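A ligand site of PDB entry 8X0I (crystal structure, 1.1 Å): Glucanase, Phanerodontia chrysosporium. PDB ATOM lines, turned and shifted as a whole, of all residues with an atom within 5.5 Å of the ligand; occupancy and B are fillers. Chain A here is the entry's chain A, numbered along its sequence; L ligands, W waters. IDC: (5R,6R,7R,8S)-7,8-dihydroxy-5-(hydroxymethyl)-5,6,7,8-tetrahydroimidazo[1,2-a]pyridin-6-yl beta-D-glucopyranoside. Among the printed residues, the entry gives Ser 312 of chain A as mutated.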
ATOM      1  N   TRP A  48     -16.848   2.944 -31.273  1.00  0.00           N
ATOM      2  CA  TRP A  48     -16.517   4.254 -30.738  1.00  0.00           C
ATOM      3  C   TRP A  48     -15.032   4.552 -30.864  1.00  0.00           C
ATOM      4  O   TRP A  48     -14.180   3.759 -30.442  1.00  0.00           O
ATOM      5  CB  TRP A  48     -16.925   4.365 -29.278  1.00  0.00           C
ATOM      6  CG  TRP A  48     -18.416   4.349 -29.073  1.00  0.00           C
ATOM      7  CD1 TRP A  48     -19.302   3.373 -29.446  1.00  0.00           C
ATOM      8  CD2 TRP A  48     -19.170   5.363 -28.412  1.00  0.00           C
ATOM      9  NE1 TRP A  48     -20.566   3.737 -29.054  1.00  0.00           N
ATOM     10  CE2 TRP A  48     -20.515   4.945 -28.416  1.00  0.00           C
ATOM     11  CE3 TRP A  48     -18.842   6.578 -27.813  1.00  0.00           C
ATOM     12  CZ2 TRP A  48     -21.528   5.692 -27.810  1.00  0.00           C
ATOM     13  CZ3 TRP A  48     -19.846   7.325 -27.218  1.00  0.00           C
ATOM     14  CH2 TRP A  48     -21.174   6.880 -27.228  1.00  0.00           C
ATOM     15  N   ASP A  50     -13.158   6.439 -29.072  1.00  0.00           N
ATOM     16  CA  ASP A  50     -13.128   7.148 -27.797  1.00  0.00           C
ATOM     17  C   ASP A  50     -11.727   7.555 -27.363  1.00  0.00           C
ATOM     18  O   ASP A  50     -11.555   8.130 -26.287  1.00  0.00           O
ATOM     19  CB  ASP A  50     -13.865   6.372 -26.693  1.00  0.00           C
ATOM     20  CG  ASP A  50     -13.231   5.022 -26.396  1.00  0.00           C
ATOM     21  OD1 ASP A  50     -12.844   4.331 -27.356  1.00  0.00           O
ATOM     22  OD2 ASP A  50     -13.132   4.656 -25.194  1.00  0.00           O
ATOM     23  N   LYS A  54      -7.842   4.258 -30.668  1.00  0.00           N
ATOM     24  CA  LYS A  54      -8.804   3.530 -31.494  1.00  0.00           C
ATOM     25  C   LYS A  54      -8.663   3.821 -32.970  1.00  0.00           C
ATOM     26  O   LYS A  54      -9.286   3.130 -33.787  1.00  0.00           O
ATOM     27  CB  LYS A  54     -10.233   3.839 -31.052  1.00  0.00           C
ATOM     28  CG  LYS A  54     -10.496   3.482 -29.599  1.00  0.00           C
ATOM     29  CD  LYS A  54     -10.283   1.997 -29.342  1.00  0.00           C
ATOM     30  CE  LYS A  54     -10.600   1.640 -27.904  1.00  0.00           C
ATOM     31  NZ  LYS A  54     -12.073   1.722 -27.672  1.00  0.00           N
ATOM     32  N   TYR A  83     -15.795  10.630 -30.574  1.00  0.00           N
ATOM     33  CA  TYR A  83     -16.049  10.821 -29.127  1.00  0.00           C
ATOM     34  C   TYR A  83     -14.731  11.067 -28.399  1.00  0.00           C
ATOM     35  O   TYR A  83     -14.254  10.247 -27.612  1.00  0.00           O
ATOM     36  CB  TYR A  83     -16.806   9.634 -28.534  1.00  0.00           C
ATOM     37  CG  TYR A  83     -17.215   9.849 -27.088  1.00  0.00           C
ATOM     38  CD1 TYR A  83     -18.008  10.927 -26.737  1.00  0.00           C
ATOM     39  CD2 TYR A  83     -16.785   8.995 -26.082  1.00  0.00           C
ATOM     40  CE1 TYR A  83     -18.378  11.149 -25.420  1.00  0.00           C
ATOM     41  CE2 TYR A  83     -17.151   9.210 -24.754  1.00  0.00           C
ATOM     42  CZ  TYR A  83     -17.950  10.290 -24.434  1.00  0.00           C
ATOM     43  OH  TYR A  83     -18.301  10.488 -23.114  1.00  0.00           O
ATOM     44  N   ARG A  88     -13.985  16.236 -22.056  1.00  0.00           N
ATOM     45  CA  ARG A  88     -15.120  15.382 -22.380  1.00  0.00           C
ATOM     46  C   ARG A  88     -15.903  15.074 -21.114  1.00  0.00           C
ATOM     47  O   ARG A  88     -15.324  14.826 -20.050  1.00  0.00           O
ATOM     48  CB  ARG A  88     -14.586  14.073 -22.981  1.00  0.00           C
ATOM     49  CG  ARG A  88     -15.605  13.297 -23.790  1.00  0.00           C
ATOM     50  CD  ARG A  88     -14.990  12.050 -24.424  1.00  0.00           C
ATOM     51  NE  ARG A  88     -14.607  11.059 -23.433  1.00  0.00           N
ATOM     52  CZ  ARG A  88     -13.876   9.991 -23.697  1.00  0.00           C
ATOM     53  NH1 ARG A  88     -13.461   9.736 -24.928  1.00  0.00           N
ATOM     54  NH2 ARG A  88     -13.542   9.165 -22.709  1.00  0.00           N
ATOM     55  N   ASP A  89     -17.236  15.085 -21.241  1.00  0.00           N
ATOM     56  CA  ASP A  89     -18.152  14.867 -20.107  1.00  0.00           C
ATOM     57  C   ASP A  89     -18.012  16.018 -19.103  1.00  0.00           C
ATOM     58  O   ASP A  89     -17.406  15.896 -18.040  1.00  0.00           O
ATOM     59  CB  ASP A  89     -17.925  13.471 -19.490  1.00  0.00           C
ATOM     60  CG  ASP A  89     -19.043  13.028 -18.561  1.00  0.00           C
ATOM     61  OD1 ASP A  89     -20.052  13.746 -18.361  1.00  0.00           O
ATOM     62  OD2 ASP A  89     -18.917  11.892 -18.026  1.00  0.00           O
ATOM     63  N   ALA A  94     -17.680  10.208 -15.180  1.00  0.00           N
ATOM     64  CA  ALA A  94     -17.448   8.808 -15.533  1.00  0.00           C
ATOM     65  C   ALA A  94     -16.741   8.649 -16.867  1.00  0.00           C
ATOM     66  O   ALA A  94     -16.022   7.666 -17.058  1.00  0.00           O
ATOM     67  CB  ALA A  94     -18.741   8.003 -15.523  1.00  0.00           C
ATOM     68  N   SER A  95     -16.939   9.583 -17.801  1.00  0.00           N
ATOM     69  CA  SER A  95     -16.413   9.457 -19.156  1.00  0.00           C
ATOM     70  C   SER A  95     -15.345  10.504 -19.459  1.00  0.00           C
ATOM     71  O   SER A  95     -15.076  10.780 -20.635  1.00  0.00           O
ATOM     72  CB  SER A  95     -17.540   9.500 -20.189  1.00  0.00           C
ATOM     73  OG  SER A  95     -18.292   8.297 -20.160  1.00  0.00           O
ATOM     74  N   PRO A 134     -21.421  12.379 -28.814  1.00  0.00           N
ATOM     75  CA  PRO A 134     -22.421  12.227 -27.749  1.00  0.00           C
ATOM     76  C   PRO A 134     -22.075  13.080 -26.539  1.00  0.00           C
ATOM     77  O   PRO A 134     -20.906  13.253 -26.192  1.00  0.00           O
ATOM     78  CB  PRO A 134     -22.362  10.726 -27.430  1.00  0.00           C
ATOM     79  CG  PRO A 134     -21.948  10.130 -28.756  1.00  0.00           C
ATOM     80  CD  PRO A 134     -20.934  11.079 -29.298  1.00  0.00           C
ATOM     81  N   ASP A 135     -23.101  13.604 -25.900  1.00  0.00           N
ATOM     82  CA  ASP A 135     -22.927  14.343 -24.657  1.00  0.00           C
ATOM     83  C   ASP A 135     -21.997  15.543 -24.828  1.00  0.00           C
ATOM     84  O   ASP A 135     -21.114  15.787 -23.993  1.00  0.00           O
ATOM     85  CB  ASP A 135     -22.455  13.422 -23.516  1.00  0.00           C
ATOM     86  CG  ASP A 135     -22.416  14.136 -22.181  1.00  0.00           C
ATOM     87  OD1 ASP A 135     -23.320  14.981 -21.950  1.00  0.00           O
ATOM     88  OD2 ASP A 135     -21.482  13.898 -21.372  1.00  0.00           O
ATOM     89  N   VAL A 217     -28.723   8.276 -27.587  1.00  0.00           N
ATOM     90  CA  VAL A 217     -27.435   7.597 -27.566  1.00  0.00           C
ATOM     91  C   VAL A 217     -27.056   7.274 -26.133  1.00  0.00           C
ATOM     92  O   VAL A 217     -26.989   8.156 -25.275  1.00  0.00           O
ATOM     93  CB  VAL A 217     -26.351   8.444 -28.246  1.00  0.00           C
ATOM     94  CG1 VAL A 217     -24.988   7.776 -28.080  1.00  0.00           C
ATOM     95  CG2 VAL A 217     -26.657   8.646 -29.709  1.00  0.00           C
ATOM     96  N   ALA A 218     -26.816   5.992 -25.865  1.00  0.00           N
ATOM     97  CA  ALA A 218     -26.469   5.497 -24.543  1.00  0.00           C
ATOM     98  C   ALA A 218     -27.607   5.642 -23.534  1.00  0.00           C
ATOM     99  O   ALA A 218     -27.381   5.411 -22.346  1.00  0.00           O
ATOM    100  CB  ALA A 218     -25.168   6.098 -23.990  1.00  0.00           C
ATOM    101  N   ARG A 266     -30.487  -0.334 -25.849  1.00  0.00           N
ATOM    102  CA  ARG A 266     -30.820  -0.707 -24.467  1.00  0.00           C
ATOM    103  C   ARG A 266     -32.226  -0.264 -24.091  1.00  0.00           C
ATOM    104  O   ARG A 266     -32.490   0.078 -22.937  1.00  0.00           O
ATOM    105  CB  ARG A 266     -29.778  -0.197 -23.474  1.00  0.00           C
ATOM    106  CG  ARG A 266     -28.380  -0.786 -23.712  1.00  0.00           C
ATOM    107  CD  ARG A 266     -27.416  -0.436 -22.591  1.00  0.00           C
ATOM    108  NE  ARG A 266     -27.138   0.995 -22.534  1.00  0.00           N
ATOM    109  CZ  ARG A 266     -26.415   1.564 -21.584  1.00  0.00           C
ATOM    110  NH1 ARG A 266     -25.779   0.855 -20.665  1.00  0.00           N
ATOM    111  NH2 ARG A 266     -26.324   2.896 -21.557  1.00  0.00           N
ATOM    112  N   TRP A 279     -28.956   7.354 -15.452  1.00  0.00           N
ATOM    113  CA  TRP A 279     -28.355   6.949 -16.717  1.00  0.00           C
ATOM    114  C   TRP A 279     -27.358   5.811 -16.589  1.00  0.00           C
ATOM    115  O   TRP A 279     -26.943   5.275 -17.619  1.00  0.00           O
ATOM    116  CB  TRP A 279     -27.644   8.153 -17.362  1.00  0.00           C
ATOM    117  CG  TRP A 279     -26.668   8.793 -16.414  1.00  0.00           C
ATOM    118  CD1 TRP A 279     -26.908   9.850 -15.576  1.00  0.00           C
ATOM    119  CD2 TRP A 279     -25.298   8.400 -16.169  1.00  0.00           C
ATOM    120  NE1 TRP A 279     -25.795  10.149 -14.839  1.00  0.00           N
ATOM    121  CE2 TRP A 279     -24.784   9.274 -15.177  1.00  0.00           C
ATOM    122  CE3 TRP A 279     -24.452   7.431 -16.705  1.00  0.00           C
ATOM    123  CZ2 TRP A 279     -23.485   9.182 -14.708  1.00  0.00           C
ATOM    124  CZ3 TRP A 279     -23.162   7.339 -16.224  1.00  0.00           C
ATOM    125  CH2 TRP A 279     -22.690   8.209 -15.238  1.00  0.00           C
ATOM    126  N   LYS A 307     -24.722   3.014 -28.477  1.00  0.00           N
ATOM    127  CA  LYS A 307     -24.017   2.508 -27.303  1.00  0.00           C
ATOM    128  C   LYS A 307     -24.023   0.989 -27.335  1.00  0.00           C
ATOM    129  O   LYS A 307     -25.090   0.381 -27.456  1.00  0.00           O
ATOM    130  CB  LYS A 307     -24.750   2.996 -26.054  1.00  0.00           C
ATOM    131  CG  LYS A 307     -24.284   2.375 -24.746  1.00  0.00           C
ATOM    132  CD  LYS A 307     -22.905   2.863 -24.297  1.00  0.00           C
ATOM    133  CE  LYS A 307     -22.457   2.115 -23.061  1.00  0.00           C
ATOM    134  NZ  LYS A 307     -21.173   2.652 -22.532  1.00  0.00           N
ATOM    135  N   PRO A 308     -22.857   0.338 -27.246  1.00  0.00           N
ATOM    136  CA  PRO A 308     -22.827  -1.132 -27.356  1.00  0.00           C
ATOM    137  C   PRO A 308     -23.171  -1.741 -26.011  1.00  0.00           C
ATOM    138  O   PRO A 308     -22.433  -1.599 -25.024  1.00  0.00           O
ATOM    139  CB  PRO A 308     -21.368  -1.415 -27.765  1.00  0.00           C
ATOM    140  CG  PRO A 308     -20.782  -0.072 -28.162  1.00  0.00           C
ATOM    141  CD  PRO A 308     -21.506   0.903 -27.267  1.00  0.00           C
ATOM    142  N   GLU A 311     -20.998  -2.663 -22.551  1.00  0.00           N
ATOM    143  CA  GLU A 311     -19.946  -1.735 -22.153  1.00  0.00           C
ATOM    144  C   GLU A 311     -20.494  -0.797 -21.092  1.00  0.00           C
ATOM    145  O   GLU A 311     -21.535  -0.158 -21.283  1.00  0.00           O
ATOM    146  CB  GLU A 311     -19.423  -0.978 -23.376  1.00  0.00           C
ATOM    147  CG  GLU A 311     -18.786  -1.911 -24.396  1.00  0.00           C
ATOM    148  CD  GLU A 311     -18.299  -1.240 -25.667  1.00  0.00           C
ATOM    149  OE1 GLU A 311     -18.334   0.015 -25.764  1.00  0.00           O
ATOM    150  OE2 GLU A 311     -17.895  -1.972 -26.598  1.00  0.00           O
ATOM    151  N   SER A 312     -19.815  -0.730 -19.957  1.00  0.00           N
ATOM    152  CA  SER A 312     -20.303   0.020 -18.806  1.00  0.00           C
ATOM    153  C   SER A 312     -20.483   1.505 -19.118  1.00  0.00           C
ATOM    154  O   SER A 312     -19.789   2.074 -19.962  1.00  0.00           O
ATOM    155  CB  SER A 312     -19.304  -0.138 -17.660  1.00  0.00           C
ATOM    156  OG  SER A 312     -19.756   0.560 -16.510  1.00  0.00           O
ATOM    157  N   ASP A 313     -21.420   2.127 -18.408  1.00  0.00           N
ATOM    158  CA  ASP A 313     -21.585   3.576 -18.445  1.00  0.00           C
ATOM    159  C   ASP A 313     -20.687   4.297 -17.446  1.00  0.00           C
ATOM    160  O   ASP A 313     -20.553   5.523 -17.532  1.00  0.00           O
ATOM    161  CB  ASP A 313     -23.025   3.969 -18.105  1.00  0.00           C
ATOM    162  CG  ASP A 313     -24.029   3.381 -19.063  1.00  0.00           C
ATOM    163  OD1 ASP A 313     -23.895   3.625 -20.290  1.00  0.00           O
ATOM    164  OD2 ASP A 313     -24.951   2.678 -18.618  1.00  0.00           O
ATOM    165  N   ARG A 322     -13.161   8.756 -11.614  1.00  0.00           N
ATOM    166  CA  ARG A 322     -14.262   8.837 -12.555  1.00  0.00           C
ATOM    167  C   ARG A 322     -15.579   8.394 -11.936  1.00  0.00           C
ATOM    168  O   ARG A 322     -16.504   8.029 -12.666  1.00  0.00           O
ATOM    169  CB  ARG A 322     -13.932   8.053 -13.827  1.00  0.00           C
ATOM    170  CG  ARG A 322     -12.671   8.565 -14.539  1.00  0.00           C
ATOM    171  CD  ARG A 322     -12.749   8.423 -16.057  1.00  0.00           C
ATOM    172  NE  ARG A 322     -12.966   7.034 -16.429  1.00  0.00           N
ATOM    173  CZ  ARG A 322     -13.286   6.626 -17.653  1.00  0.00           C
ATOM    174  NH1 ARG A 322     -13.334   7.463 -18.673  1.00  0.00           N
ATOM    175  NH2 ARG A 322     -13.579   5.345 -17.847  1.00  0.00           N
ATOM    176  N   ALA A 339     -16.306   3.160 -17.212  1.00  0.00           N
ATOM    177  CA  ALA A 339     -17.040   3.441 -18.444  1.00  0.00           C
ATOM    178  C   ALA A 339     -16.281   2.928 -19.648  1.00  0.00           C
ATOM    179  O   ALA A 339     -15.063   3.128 -19.776  1.00  0.00           O
ATOM    180  CB  ALA A 339     -17.281   4.938 -18.599  1.00  0.00           C
ATOM    181  N   GLY A 340     -17.008   2.262 -20.543  1.00  0.00           N
ATOM    182  CA  GLY A 340     -16.456   1.692 -21.754  1.00  0.00           C
ATOM    183  C   GLY A 340     -15.944   0.270 -21.614  1.00  0.00           C
ATOM    184  O   GLY A 340     -15.835  -0.437 -22.624  1.00  0.00           O
HETATM  185  C1  IDC L   1     -18.812   5.950 -23.166  1.00  0.00           C
HETATM  186  C2  IDC L   1     -17.433   5.616 -22.699  1.00  0.00           C
HETATM  187  C3  IDC L   1     -16.554   5.259 -23.858  1.00  0.00           C
HETATM  188  C4  IDC L   1     -17.136   4.157 -24.706  1.00  0.00           C
HETATM  189  C5  IDC L   1     -18.607   4.415 -25.033  1.00  0.00           C
HETATM  190  C6  IDC L   1     -19.291   3.206 -25.608  1.00  0.00           C
HETATM  191  O2  IDC L   1     -16.889   6.775 -22.036  1.00  0.00           O
HETATM  192  O3  IDC L   1     -15.257   4.861 -23.367  1.00  0.00           O
HETATM  193  O4  IDC L   1     -16.406   4.092 -25.931  1.00  0.00           O
HETATM  194  O5  IDC L   1     -19.338   4.737 -23.807  1.00  0.00           O
HETATM  195  O6  IDC L   1     -19.380   2.182 -24.655  1.00  0.00           O
HETATM  196  C1B IDC L   1     -22.448   8.717 -20.855  1.00  0.00           C
HETATM  197  C2B IDC L   1     -22.984   7.273 -21.089  1.00  0.00           C
HETATM  198  C3B IDC L   1     -21.822   6.389 -21.296  1.00  0.00           C
HETATM  199  C4B IDC L   1     -20.878   6.812 -22.410  1.00  0.00           C
HETATM  200  C5B IDC L   1     -20.664   8.293 -22.585  1.00  0.00           C
HETATM  201  C6B IDC L   1     -21.214   8.795 -23.970  1.00  0.00           C
HETATM  202  O2B IDC L   1     -23.690   6.926 -19.873  1.00  0.00           O
HETATM  203  O3B IDC L   1     -22.271   5.075 -21.663  1.00  0.00           O
HETATM  204  O1  IDC L   1     -19.606   6.193 -22.070  1.00  0.00           O
HETATM  205  N1B IDC L   1     -21.342   9.164 -21.536  1.00  0.00           N
HETATM  206  O6B IDC L   1     -22.555   8.395 -24.103  1.00  0.00           O
HETATM  207  N2B IDC L   1     -22.854   9.685 -20.031  1.00  0.00           N
HETATM  208  C7B IDC L   1     -22.046  10.760 -20.201  1.00  0.00           C
HETATM  209  C8B IDC L   1     -21.095  10.413 -21.164  1.00  0.00           C
HETATM  210  O   HOH W   1     -13.946   1.718 -25.274  1.00  0.00           O
HETATM  211  O   HOH W   2     -25.057  10.489 -18.504  1.00  0.00           O
HETATM  212  O   HOH W   3     -16.292   1.452 -26.815  1.00  0.00           O
HETATM  213  O   HOH W   4     -25.302  10.007 -22.155  1.00  0.00           O
HETATM  214  O   HOH W   5     -20.480   8.206 -18.525  1.00  0.00           O
HETATM  215  O   HOH W   6     -24.904  10.039 -25.052  1.00  0.00           O
HETATM  216  O   HOH W   7     -14.417   6.361 -20.926  1.00  0.00           O
HETATM  217  O   HOH W   8     -19.265  12.912 -22.507  1.00  0.00           O
HETATM  218  O   HOH W   9     -12.361   6.536 -23.197  1.00  0.00           O
HETATM  219  O   HOH W  10     -26.302   6.414 -20.100  1.00  0.00           O
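Water W10 lies within hydrogen-bond range of an oxygen (O2B) of the ligand, the backbone carbonyl oxygen (O) of Ala 218 and the backbone carbonyl oxygen (O) of Trp 279. Water W7 lies within hydrogen-bond range of NH1 of Arg 322 (2.7 Å), O2 of the ligand (2.7 Å), NH2 of Arg 88 (3.4 Å) and O of Ala 339 (3.5 Å). Water W3 lies within hydrogen-bond range of OE1 of Glu 311 (2.7 Å) and O4 of the ligand (2.8 Å). Water W6 lies within hydrogen-bond range of the backbone carbonyl oxygen of Val 217 (2.8 Å) and an oxygen (O6B) of the ligand (3.0 Å). Water W9 lies within hydrogen-bond range of OD2 of Asp 50, NH2 of Arg 88 and O3 of the ligand. Water W1 lies within hydrogen-bond range of NZ of Lys 54 (3.0 Å), OD2 of Asp 50 (3.0 Å) and O4 of the ligand (3.5 Å).
Residues that only touch the ligand: Trp 48, Tyr 83, Asp 89, Asp 135, Ala 218, Trp 279, Pro 308, Ala 339 and Gly 340. Hydrophobic or aromatic side chains within 4 Å of the ligand: Trp 48, Tyr 83, Ala 218, Trp 279, Pro 308 and Ala 339. 14 residues have an atom within 4 Å of the ligand: Trp 48, Asp 50, Tyr 83, Asp 89, Ser 95, Asp 135, Ala 218, Trp 279, Lys 307, Pro 308, Glu 311, Asp 313, Ala 339 and Gly 340. Along chain A the residues within 4 Å of the ligand span positions 48 to 340.
The side-chain carboxylate (OD1) of Asp 313 is in salt-bridge range of the guanidinium group (NH2) of Arg 266, 2.8 Å away. O of Glu 311 sits close to NZ of Lys 307 (3.1 Å). N of Ser 95 is in hydrogen-bond range of OD2 of Asp 89 (3.0 Å). NZ of Lys 54 is in salt-bridge range of OD1 of Asp 50 (2.7 Å). The backbone carbonyl oxygen (O) of Tyr 83 sits at hydrogen-bond distance from the guanidinium group (NH1) of Arg 88 (2.8 Å). NH2 of Arg 266 is in hydrogen-bond range of O of Ala 218, 2.8 Å away. The backbone NH (N) of Gly 340 lies within hydrogen-bond range of the backbone carbonyl oxygen (O) of Ser 312, at 2.8 Å. O of Ala 339 lies within hydrogen-bond range of NH2 of Arg 322 (3.3 Å).
O3B of the ligand sits at hydrogen-bond distance from OD1 of Asp 313 (2.6 Å). The side-chain carboxylate (OE1) of Glu 311 sits at hydrogen-bond distance from an oxygen (O6) of the ligand (2.6 Å). OG of Ser 95 sits at hydrogen-bond distance from O2 of the ligand (2.8 Å). An oxygen (O3B) of the ligand is in hydrogen-bond range of the side-chain amino group (NZ) of Lys 307 (2.8 Å). O3 of the ligand sits at hydrogen-bond distance from OD2 of Asp 50 (2.8 Å).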
